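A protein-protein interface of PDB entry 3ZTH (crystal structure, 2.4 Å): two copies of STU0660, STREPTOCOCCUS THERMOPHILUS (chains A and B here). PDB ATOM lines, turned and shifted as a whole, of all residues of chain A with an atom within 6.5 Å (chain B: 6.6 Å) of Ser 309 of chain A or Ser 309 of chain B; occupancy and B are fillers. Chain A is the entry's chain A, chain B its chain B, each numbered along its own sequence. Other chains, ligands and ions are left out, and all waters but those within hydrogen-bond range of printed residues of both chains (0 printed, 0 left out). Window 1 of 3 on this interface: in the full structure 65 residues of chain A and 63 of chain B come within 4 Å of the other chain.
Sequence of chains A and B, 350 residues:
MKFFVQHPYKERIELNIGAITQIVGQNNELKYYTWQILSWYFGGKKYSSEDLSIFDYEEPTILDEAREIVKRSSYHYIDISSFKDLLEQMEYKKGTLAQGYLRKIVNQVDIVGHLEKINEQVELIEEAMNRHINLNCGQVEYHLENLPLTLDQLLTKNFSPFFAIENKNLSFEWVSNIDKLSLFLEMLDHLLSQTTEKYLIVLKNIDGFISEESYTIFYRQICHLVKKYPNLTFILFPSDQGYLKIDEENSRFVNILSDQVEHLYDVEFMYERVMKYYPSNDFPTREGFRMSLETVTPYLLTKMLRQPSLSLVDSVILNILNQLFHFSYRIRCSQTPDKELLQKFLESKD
Among the printed residues, merely in contact across the chains: Gln 241 of chain A with Gln 241 of chain B (3.1 Å), Ser 309 of chain A with Leu 310 of chain B (3.5 Å), Leu 310 of chain A with Leu 310 of chain B (3.6 Å), Leu 310 of chain A with Ser 309 of chain B (3.6 Å), Ser 311 of chain A with Leu 310 of chain B (3.7 Å) and Ser 309 of chain A with Thr 295 of chain B (3.8 Å).
Of the 12 printed residues of chain B, 6 touch a printed residue of chain A. Hydrophobic or aromatic side chains of chain B that line the printed part of chain A: Leu 310. Along chain B the printed residues that touch a printed residue of chain A span positions 241 to 314. Of the 11 printed residues of chain A, 5 touch a printed residue of chain B. Hydrophobic or aromatic side chains of chain A within 4 Å of the printed part of chain B: Leu 310. Among the printed residues, no Asp or Glu carboxylate lies within 4 Å of a Lys or Arg side-chain nitrogen of the other chain.
The side-chain hydroxyl of Ser 309 of chain A is in hydrogen-bond range of the backbone NH of Ser 311 of chain B, 2.9 Å away. The side-chain hydroxyl of Ser 309 of chain A lies within hydrogen-bond range of the side-chain carboxylate of Asp 314 of chain B (2.5 Å). O of Leu 310 of chain A lies close to N of Ser 311 of chain B (3.4 Å). The backbone NH (N) of Ser 311 of chain A lies within hydrogen-bond range of the side-chain hydroxyl (OG) of Ser 309 of chain B, 2.9 Å away. OG of Ser 309 of chain B lies within hydrogen-bond range of OD2 of Asp 314 of chain A. O of Ser 309 of chain A lies close to O of Ser 309 of chain B (3.3 Å).
Gln 241 of chain A touches its own counterpart, Gln 241 of chain B. Ser 309 of chain A touches Leu 310 of chain B, and with the chains exchanged Leu 310 of chain A touches Ser 309 of chain B. Leu 310 of chain A touches its own counterpart, Leu 310 of chain B. Leu 310 of chain A touches Ser 311 of chain B, and with the chains exchanged Ser 311 of chain A touches Leu 310 of chain B. Positions printed for both chains: 241, 295, 306, 307, 308, 309, 310, 311, 312, 314 and 315.
The side-chain hydroxyl (OG) of Ser 311 of chain A sits at hydrogen-bond distance from the backbone NH (N) of Asp 314 of chain A (3.1 Å). The backbone carbonyl oxygen (O) of Ser 311 of chain A sits at hydrogen-bond distance from the side-chain hydroxyl (OG) of Ser 315 of chain A (2.8 Å). The side-chain hydroxyl (OG) of Ser 311 of chain B lies within hydrogen-bond range of the side-chain carboxylate (OD2) of Asp 314 of chain B. OG of Ser 315 of chain B sits at hydrogen-bond distance from O of Ser 311 of chain B (2.9 Å).
Of chain B, only Thr 295 (3.8 Å), Ser 309 (3.3 Å), Leu 310 (3.5 Å), Ser 311 (2.9 Å) and Asp 314 (2.5 Å) come within 4 Å of Ser 309 of chain A. Of the printed residues of chain B, Ser 311 of chain A touches Ser 309 (2.9 Å) and Leu 310 (3.7 Å). Of the printed residues of chain B, Asp 314 of chain A touches Ser 309 (2.8 Å). Of chain A, only Ser 309 (3.3 Å), Leu 310 (3.6 Å), Ser 311 (2.9 Å) and Asp 314 (2.8 Å) come within 4 Å of Ser 309 of chain B. Of the printed residues of chain A, Ser 311 of chain B touches Ser 309 (2.9 Å) and Leu 310 (3.3 Å). The nearest printed residue of chain B that does not touch Leu 310 of chain A is Leu 312 of chain B (5.1 Å).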
ATOM      1  N   GLN A 241     -26.712  10.161  18.957  1.00  0.00           N
ATOM      2  CA  GLN A 241     -26.391  10.906  17.749  1.00  0.00           C
ATOM      3  C   GLN A 241     -26.940  12.321  17.623  1.00  0.00           C
ATOM      4  O   GLN A 241     -28.092  12.587  17.931  1.00  0.00           O
ATOM      5  CB  GLN A 241     -26.811  10.073  16.528  1.00  0.00           C
ATOM      6  CG  GLN A 241     -26.481  10.703  15.176  1.00  0.00           C
ATOM      7  CD  GLN A 241     -27.568  11.657  14.673  1.00  0.00           C
ATOM      8  OE1 GLN A 241     -27.285  12.612  13.935  1.00  0.00           O
ATOM      9  NE2 GLN A 241     -28.818  11.392  15.058  1.00  0.00           N
ATOM     10  N   THR A 295     -19.335  12.110  16.583  1.00  0.00           N
ATOM     11  CA  THR A 295     -20.156  11.041  16.040  1.00  0.00           C
ATOM     12  C   THR A 295     -19.913   9.687  16.699  1.00  0.00           C
ATOM     13  O   THR A 295     -20.848   8.987  17.069  1.00  0.00           O
ATOM     14  CB  THR A 295     -19.874  10.862  14.536  1.00  0.00           C
ATOM     15  OG1 THR A 295     -20.275  12.043  13.832  1.00  0.00           O
ATOM     16  CG2 THR A 295     -20.608   9.638  13.988  1.00  0.00           C
ATOM     17  N   ARG A 306     -24.135  -5.729  16.617  1.00  0.00           N
ATOM     18  CA  ARG A 306     -24.417  -5.215  15.283  1.00  0.00           C
ATOM     19  C   ARG A 306     -23.504  -4.026  15.039  1.00  0.00           C
ATOM     20  O   ARG A 306     -23.440  -3.123  15.867  1.00  0.00           O
ATOM     21  CB  ARG A 306     -25.866  -4.736  15.185  1.00  0.00           C
ATOM     22  CG  ARG A 306     -26.919  -5.806  15.398  1.00  0.00           C
ATOM     23  CD  ARG A 306     -28.315  -5.190  15.409  1.00  0.00           C
ATOM     24  NE  ARG A 306     -29.355  -6.187  15.166  1.00  0.00           N
ATOM     25  CZ  ARG A 306     -30.656  -5.917  15.101  1.00  0.00           C
ATOM     26  NH1 ARG A 306     -31.094  -4.673  15.265  1.00  0.00           N
ATOM     27  NH2 ARG A 306     -31.522  -6.893  14.857  1.00  0.00           N
ATOM     28  N   GLN A 307     -22.804  -4.019  13.909  1.00  0.00           N
ATOM     29  CA  GLN A 307     -21.914  -2.910  13.582  1.00  0.00           C
ATOM     30  C   GLN A 307     -22.712  -1.659  13.303  1.00  0.00           C
ATOM     31  O   GLN A 307     -23.588  -1.662  12.441  1.00  0.00           O
ATOM     32  CB  GLN A 307     -21.096  -3.210  12.337  1.00  0.00           C
ATOM     33  CG  GLN A 307     -19.894  -4.061  12.574  1.00  0.00           C
ATOM     34  CD  GLN A 307     -18.869  -3.873  11.484  1.00  0.00           C
ATOM     35  OE1 GLN A 307     -17.784  -4.456  11.532  1.00  0.00           O
ATOM     36  NE2 GLN A 307     -19.204  -3.050  10.489  1.00  0.00           N
ATOM     37  N   PRO A 308     -22.420  -0.563  14.020  1.00  0.00           N
ATOM     38  CA  PRO A 308     -23.178   0.663  13.759  1.00  0.00           C
ATOM     39  C   PRO A 308     -22.859   1.147  12.353  1.00  0.00           C
ATOM     40  O   PRO A 308     -21.739   0.978  11.869  1.00  0.00           O
ATOM     41  CB  PRO A 308     -22.685   1.616  14.846  1.00  0.00           C
ATOM     42  CG  PRO A 308     -21.271   1.177  15.048  1.00  0.00           C
ATOM     43  CD  PRO A 308     -21.387  -0.336  15.046  1.00  0.00           C
ATOM     44  N   SER A 309     -23.860   1.715  11.691  1.00  0.00           N
ATOM     45  CA  SER A 309     -23.694   2.227  10.341  1.00  0.00           C
ATOM     46  C   SER A 309     -22.897   3.522  10.438  1.00  0.00           C
ATOM     47  O   SER A 309     -23.332   4.488  11.077  1.00  0.00           O
ATOM     48  CB  SER A 309     -25.062   2.489   9.699  1.00  0.00           C
ATOM     49  OG  SER A 309     -24.929   2.823   8.328  1.00  0.00           O
ATOM     50  N   LEU A 310     -21.725   3.531   9.812  1.00  0.00           N
ATOM     51  CA  LEU A 310     -20.869   4.701   9.845  1.00  0.00           C
ATOM     52  C   LEU A 310     -20.138   4.883   8.530  1.00  0.00           C
ATOM     53  O   LEU A 310     -20.010   3.939   7.744  1.00  0.00           O
ATOM     54  CB  LEU A 310     -19.831   4.574  10.964  1.00  0.00           C
ATOM     55  CG  LEU A 310     -20.315   4.442  12.406  1.00  0.00           C
ATOM     56  CD1 LEU A 310     -19.117   4.192  13.325  1.00  0.00           C
ATOM     57  CD2 LEU A 310     -21.062   5.702  12.811  1.00  0.00           C
ATOM     58  N   SER A 311     -19.664   6.105   8.300  1.00  0.00           N
ATOM     59  CA  SER A 311     -18.906   6.416   7.101  1.00  0.00           C
ATOM     60  C   SER A 311     -17.553   5.727   7.255  1.00  0.00           C
ATOM     61  O   SER A 311     -17.146   5.367   8.360  1.00  0.00           O
ATOM     62  CB  SER A 311     -18.697   7.925   6.963  1.00  0.00           C
ATOM     63  OG  SER A 311     -17.797   8.411   7.950  1.00  0.00           O
ATOM     64  N   LEU A 312     -16.866   5.546   6.138  1.00  0.00           N
ATOM     65  CA  LEU A 312     -15.567   4.910   6.128  1.00  0.00           C
ATOM     66  C   LEU A 312     -14.600   5.628   7.083  1.00  0.00           C
ATOM     67  O   LEU A 312     -13.893   4.993   7.870  1.00  0.00           O
ATOM     68  CB  LEU A 312     -15.037   4.910   4.690  1.00  0.00           C
ATOM     69  CG  LEU A 312     -13.714   4.211   4.357  1.00  0.00           C
ATOM     70  CD1 LEU A 312     -13.657   2.806   4.977  1.00  0.00           C
ATOM     71  CD2 LEU A 312     -13.571   4.157   2.831  1.00  0.00           C
ATOM     72  N   ASP A 314     -15.327   7.721   9.683  1.00  0.00           N
ATOM     73  CA  ASP A 314     -15.705   7.635  11.079  1.00  0.00           C
ATOM     74  C   ASP A 314     -15.381   6.254  11.643  1.00  0.00           C
ATOM     75  O   ASP A 314     -15.024   6.127  12.820  1.00  0.00           O
ATOM     76  CB  ASP A 314     -17.195   7.962  11.261  1.00  0.00           C
ATOM     77  CG  ASP A 314     -17.501   9.453  11.066  1.00  0.00           C
ATOM     78  OD1 ASP A 314     -16.564  10.282  11.096  1.00  0.00           O
ATOM     79  OD2 ASP A 314     -18.689   9.805  10.894  1.00  0.00           O
ATOM     80  N   SER A 315     -15.486   5.226  10.802  1.00  0.00           N
ATOM     81  CA  SER A 315     -15.203   3.852  11.228  1.00  0.00           C
ATOM     82  C   SER A 315     -13.728   3.731  11.572  1.00  0.00           C
ATOM     83  O   SER A 315     -13.355   3.067  12.536  1.00  0.00           O
ATOM     84  CB  SER A 315     -15.544   2.857  10.117  1.00  0.00           C
ATOM     85  OG  SER A 315     -16.903   2.952   9.739  1.00  0.00           O
ATOM     86  N   GLN B 241     -31.623   5.480  16.658  1.00  0.00           N
ATOM     87  CA  GLN B 241     -30.735   4.355  16.382  1.00  0.00           C
ATOM     88  C   GLN B 241     -30.864   3.103  17.248  1.00  0.00           C
ATOM     89  O   GLN B 241     -30.838   3.176  18.476  1.00  0.00           O
ATOM     90  CB  GLN B 241     -29.285   4.852  16.444  1.00  0.00           C
ATOM     91  CG  GLN B 241     -29.007   6.068  15.541  1.00  0.00           C
ATOM     92  CD  GLN B 241     -27.708   6.812  15.871  1.00  0.00           C
ATOM     93  OE1 GLN B 241     -27.101   7.434  14.993  1.00  0.00           O
ATOM     94  NE2 GLN B 241     -27.293   6.767  17.137  1.00  0.00           N
ATOM     95  N   THR B 295     -32.305   1.144  10.067  1.00  0.00           N
ATOM     96  CA  THR B 295     -31.280   2.148  10.298  1.00  0.00           C
ATOM     97  C   THR B 295     -31.642   3.510   9.733  1.00  0.00           C
ATOM     98  O   THR B 295     -31.571   4.525  10.417  1.00  0.00           O
ATOM     99  CB  THR B 295     -29.931   1.733   9.666  1.00  0.00           C
ATOM    100  OG1 THR B 295     -29.469   0.522  10.271  1.00  0.00           O
ATOM    101  CG2 THR B 295     -28.883   2.815   9.875  1.00  0.00           C
ATOM    102  N   VAL B 296     -32.051   3.501   8.476  1.00  0.00           N
ATOM    103  CA  VAL B 296     -32.355   4.698   7.714  1.00  0.00           C
ATOM    104  C   VAL B 296     -33.702   5.397   7.911  1.00  0.00           C
ATOM    105  O   VAL B 296     -33.794   6.631   7.827  1.00  0.00           O
ATOM    106  CB  VAL B 296     -32.133   4.354   6.215  1.00  0.00           C
ATOM    107  CG1 VAL B 296     -33.024   5.178   5.315  1.00  0.00           C
ATOM    108  CG2 VAL B 296     -30.664   4.555   5.874  1.00  0.00           C
ATOM    109  N   ARG B 306     -26.655  18.800   8.633  1.00  0.00           N
ATOM    110  CA  ARG B 306     -25.475  17.971   8.855  1.00  0.00           C
ATOM    111  C   ARG B 306     -25.748  16.577   8.294  1.00  0.00           C
ATOM    112  O   ARG B 306     -26.542  15.822   8.853  1.00  0.00           O
ATOM    113  CB  ARG B 306     -25.177  17.875  10.354  1.00  0.00           C
ATOM    114  CG  ARG B 306     -25.130  19.224  11.054  1.00  0.00           C
ATOM    115  CD  ARG B 306     -25.432  19.099  12.543  1.00  0.00           C
ATOM    116  NE  ARG B 306     -25.994  20.340  13.077  1.00  0.00           N
ATOM    117  CZ  ARG B 306     -26.452  20.487  14.319  1.00  0.00           C
ATOM    118  NH1 ARG B 306     -26.417  19.465  15.167  1.00  0.00           N
ATOM    119  NH2 ARG B 306     -26.949  21.659  14.710  1.00  0.00           N
ATOM    120  N   GLN B 307     -25.101  16.242   7.184  1.00  0.00           N
ATOM    121  CA  GLN B 307     -25.287  14.932   6.567  1.00  0.00           C
ATOM    122  C   GLN B 307     -24.961  13.821   7.570  1.00  0.00           C
ATOM    123  O   GLN B 307     -23.908  13.839   8.208  1.00  0.00           O
ATOM    124  CB  GLN B 307     -24.398  14.814   5.331  1.00  0.00           C
ATOM    125  CG  GLN B 307     -24.549  13.512   4.588  1.00  0.00           C
ATOM    126  CD  GLN B 307     -23.784  13.504   3.279  1.00  0.00           C
ATOM    127  OE1 GLN B 307     -24.170  14.166   2.309  1.00  0.00           O
ATOM    128  NE2 GLN B 307     -22.686  12.758   3.247  1.00  0.00           N
ATOM    129  N   PRO B 308     -25.865  12.840   7.729  1.00  0.00           N
ATOM    130  CA  PRO B 308     -25.609  11.753   8.682  1.00  0.00           C
ATOM    131  C   PRO B 308     -24.522  10.780   8.241  1.00  0.00           C
ATOM    132  O   PRO B 308     -24.329  10.537   7.047  1.00  0.00           O
ATOM    133  CB  PRO B 308     -26.976  11.080   8.811  1.00  0.00           C
ATOM    134  CG  PRO B 308     -27.546  11.235   7.427  1.00  0.00           C
ATOM    135  CD  PRO B 308     -27.178  12.675   7.074  1.00  0.00           C
ATOM    136  N   SER B 309     -23.799  10.240   9.218  1.00  0.00           N
ATOM    137  CA  SER B 309     -22.747   9.279   8.933  1.00  0.00           C
ATOM    138  C   SER B 309     -23.403   7.910   8.771  1.00  0.00           C
ATOM    139  O   SER B 309     -24.000   7.391   9.710  1.00  0.00           O
ATOM    140  CB  SER B 309     -21.730   9.246  10.078  1.00  0.00           C
ATOM    141  OG  SER B 309     -20.728   8.270   9.847  1.00  0.00           O
ATOM    142  N   LEU B 310     -23.294   7.339   7.576  1.00  0.00           N
ATOM    143  CA  LEU B 310     -23.881   6.038   7.279  1.00  0.00           C
ATOM    144  C   LEU B 310     -23.005   5.245   6.331  1.00  0.00           C
ATOM    145  O   LEU B 310     -22.249   5.813   5.543  1.00  0.00           O
ATOM    146  CB  LEU B 310     -25.253   6.206   6.622  1.00  0.00           C
ATOM    147  CG  LEU B 310     -26.413   6.792   7.426  1.00  0.00           C
ATOM    148  CD1 LEU B 310     -27.570   7.016   6.482  1.00  0.00           C
ATOM    149  CD2 LEU B 310     -26.809   5.852   8.567  1.00  0.00           C
ATOM    150  N   SER B 311     -23.114   3.926   6.396  1.00  0.00           N
ATOM    151  CA  SER B 311     -22.337   3.083   5.499  1.00  0.00           C
ATOM    152  C   SER B 311     -22.773   3.425   4.078  1.00  0.00           C
ATOM    153  O   SER B 311     -23.809   4.074   3.864  1.00  0.00           O
ATOM    154  CB  SER B 311     -22.603   1.605   5.778  1.00  0.00           C
ATOM    155  OG  SER B 311     -23.952   1.280   5.511  1.00  0.00           O
ATOM    156  N   LEU B 312     -21.983   2.984   3.109  1.00  0.00           N
ATOM    157  CA  LEU B 312     -22.273   3.253   1.713  1.00  0.00           C
ATOM    158  C   LEU B 312     -23.638   2.698   1.279  1.00  0.00           C
ATOM    159  O   LEU B 312     -24.386   3.370   0.570  1.00  0.00           O
ATOM    160  CB  LEU B 312     -21.154   2.673   0.850  1.00  0.00           C
ATOM    161  CG  LEU B 312     -21.156   3.008  -0.640  1.00  0.00           C
ATOM    162  CD1 LEU B 312     -21.308   4.504  -0.844  1.00  0.00           C
ATOM    163  CD2 LEU B 312     -19.854   2.529  -1.255  1.00  0.00           C
ATOM    164  N   ASP B 314     -26.404   1.892   3.222  1.00  0.00           N
ATOM    165  CA  ASP B 314     -27.521   2.568   3.861  1.00  0.00           C
ATOM    166  C   ASP B 314     -27.783   3.919   3.205  1.00  0.00           C
ATOM    167  O   ASP B 314     -28.932   4.327   3.040  1.00  0.00           O
ATOM    168  CB  ASP B 314     -27.260   2.757   5.365  1.00  0.00           C
ATOM    169  CG  ASP B 314     -27.205   1.434   6.124  1.00  0.00           C
ATOM    170  OD1 ASP B 314     -27.762   0.430   5.629  1.00  0.00           O
ATOM    171  OD2 ASP B 314     -26.613   1.396   7.223  1.00  0.00           O
ATOM    172  N   SER B 315     -26.714   4.608   2.823  1.00  0.00           N
ATOM    173  CA  SER B 315     -26.848   5.910   2.186  1.00  0.00           C
ATOM    174  C   SER B 315     -27.580   5.788   0.853  1.00  0.00           C
ATOM    175  O   SER B 315     -28.458   6.602   0.548  1.00  0.00           O
ATOM    176  CB  SER B 315     -25.475   6.533   1.956  1.00  0.00           C
ATOM    177  OG  SER B 315     -24.797   6.718   3.176  1.00  0.00           O
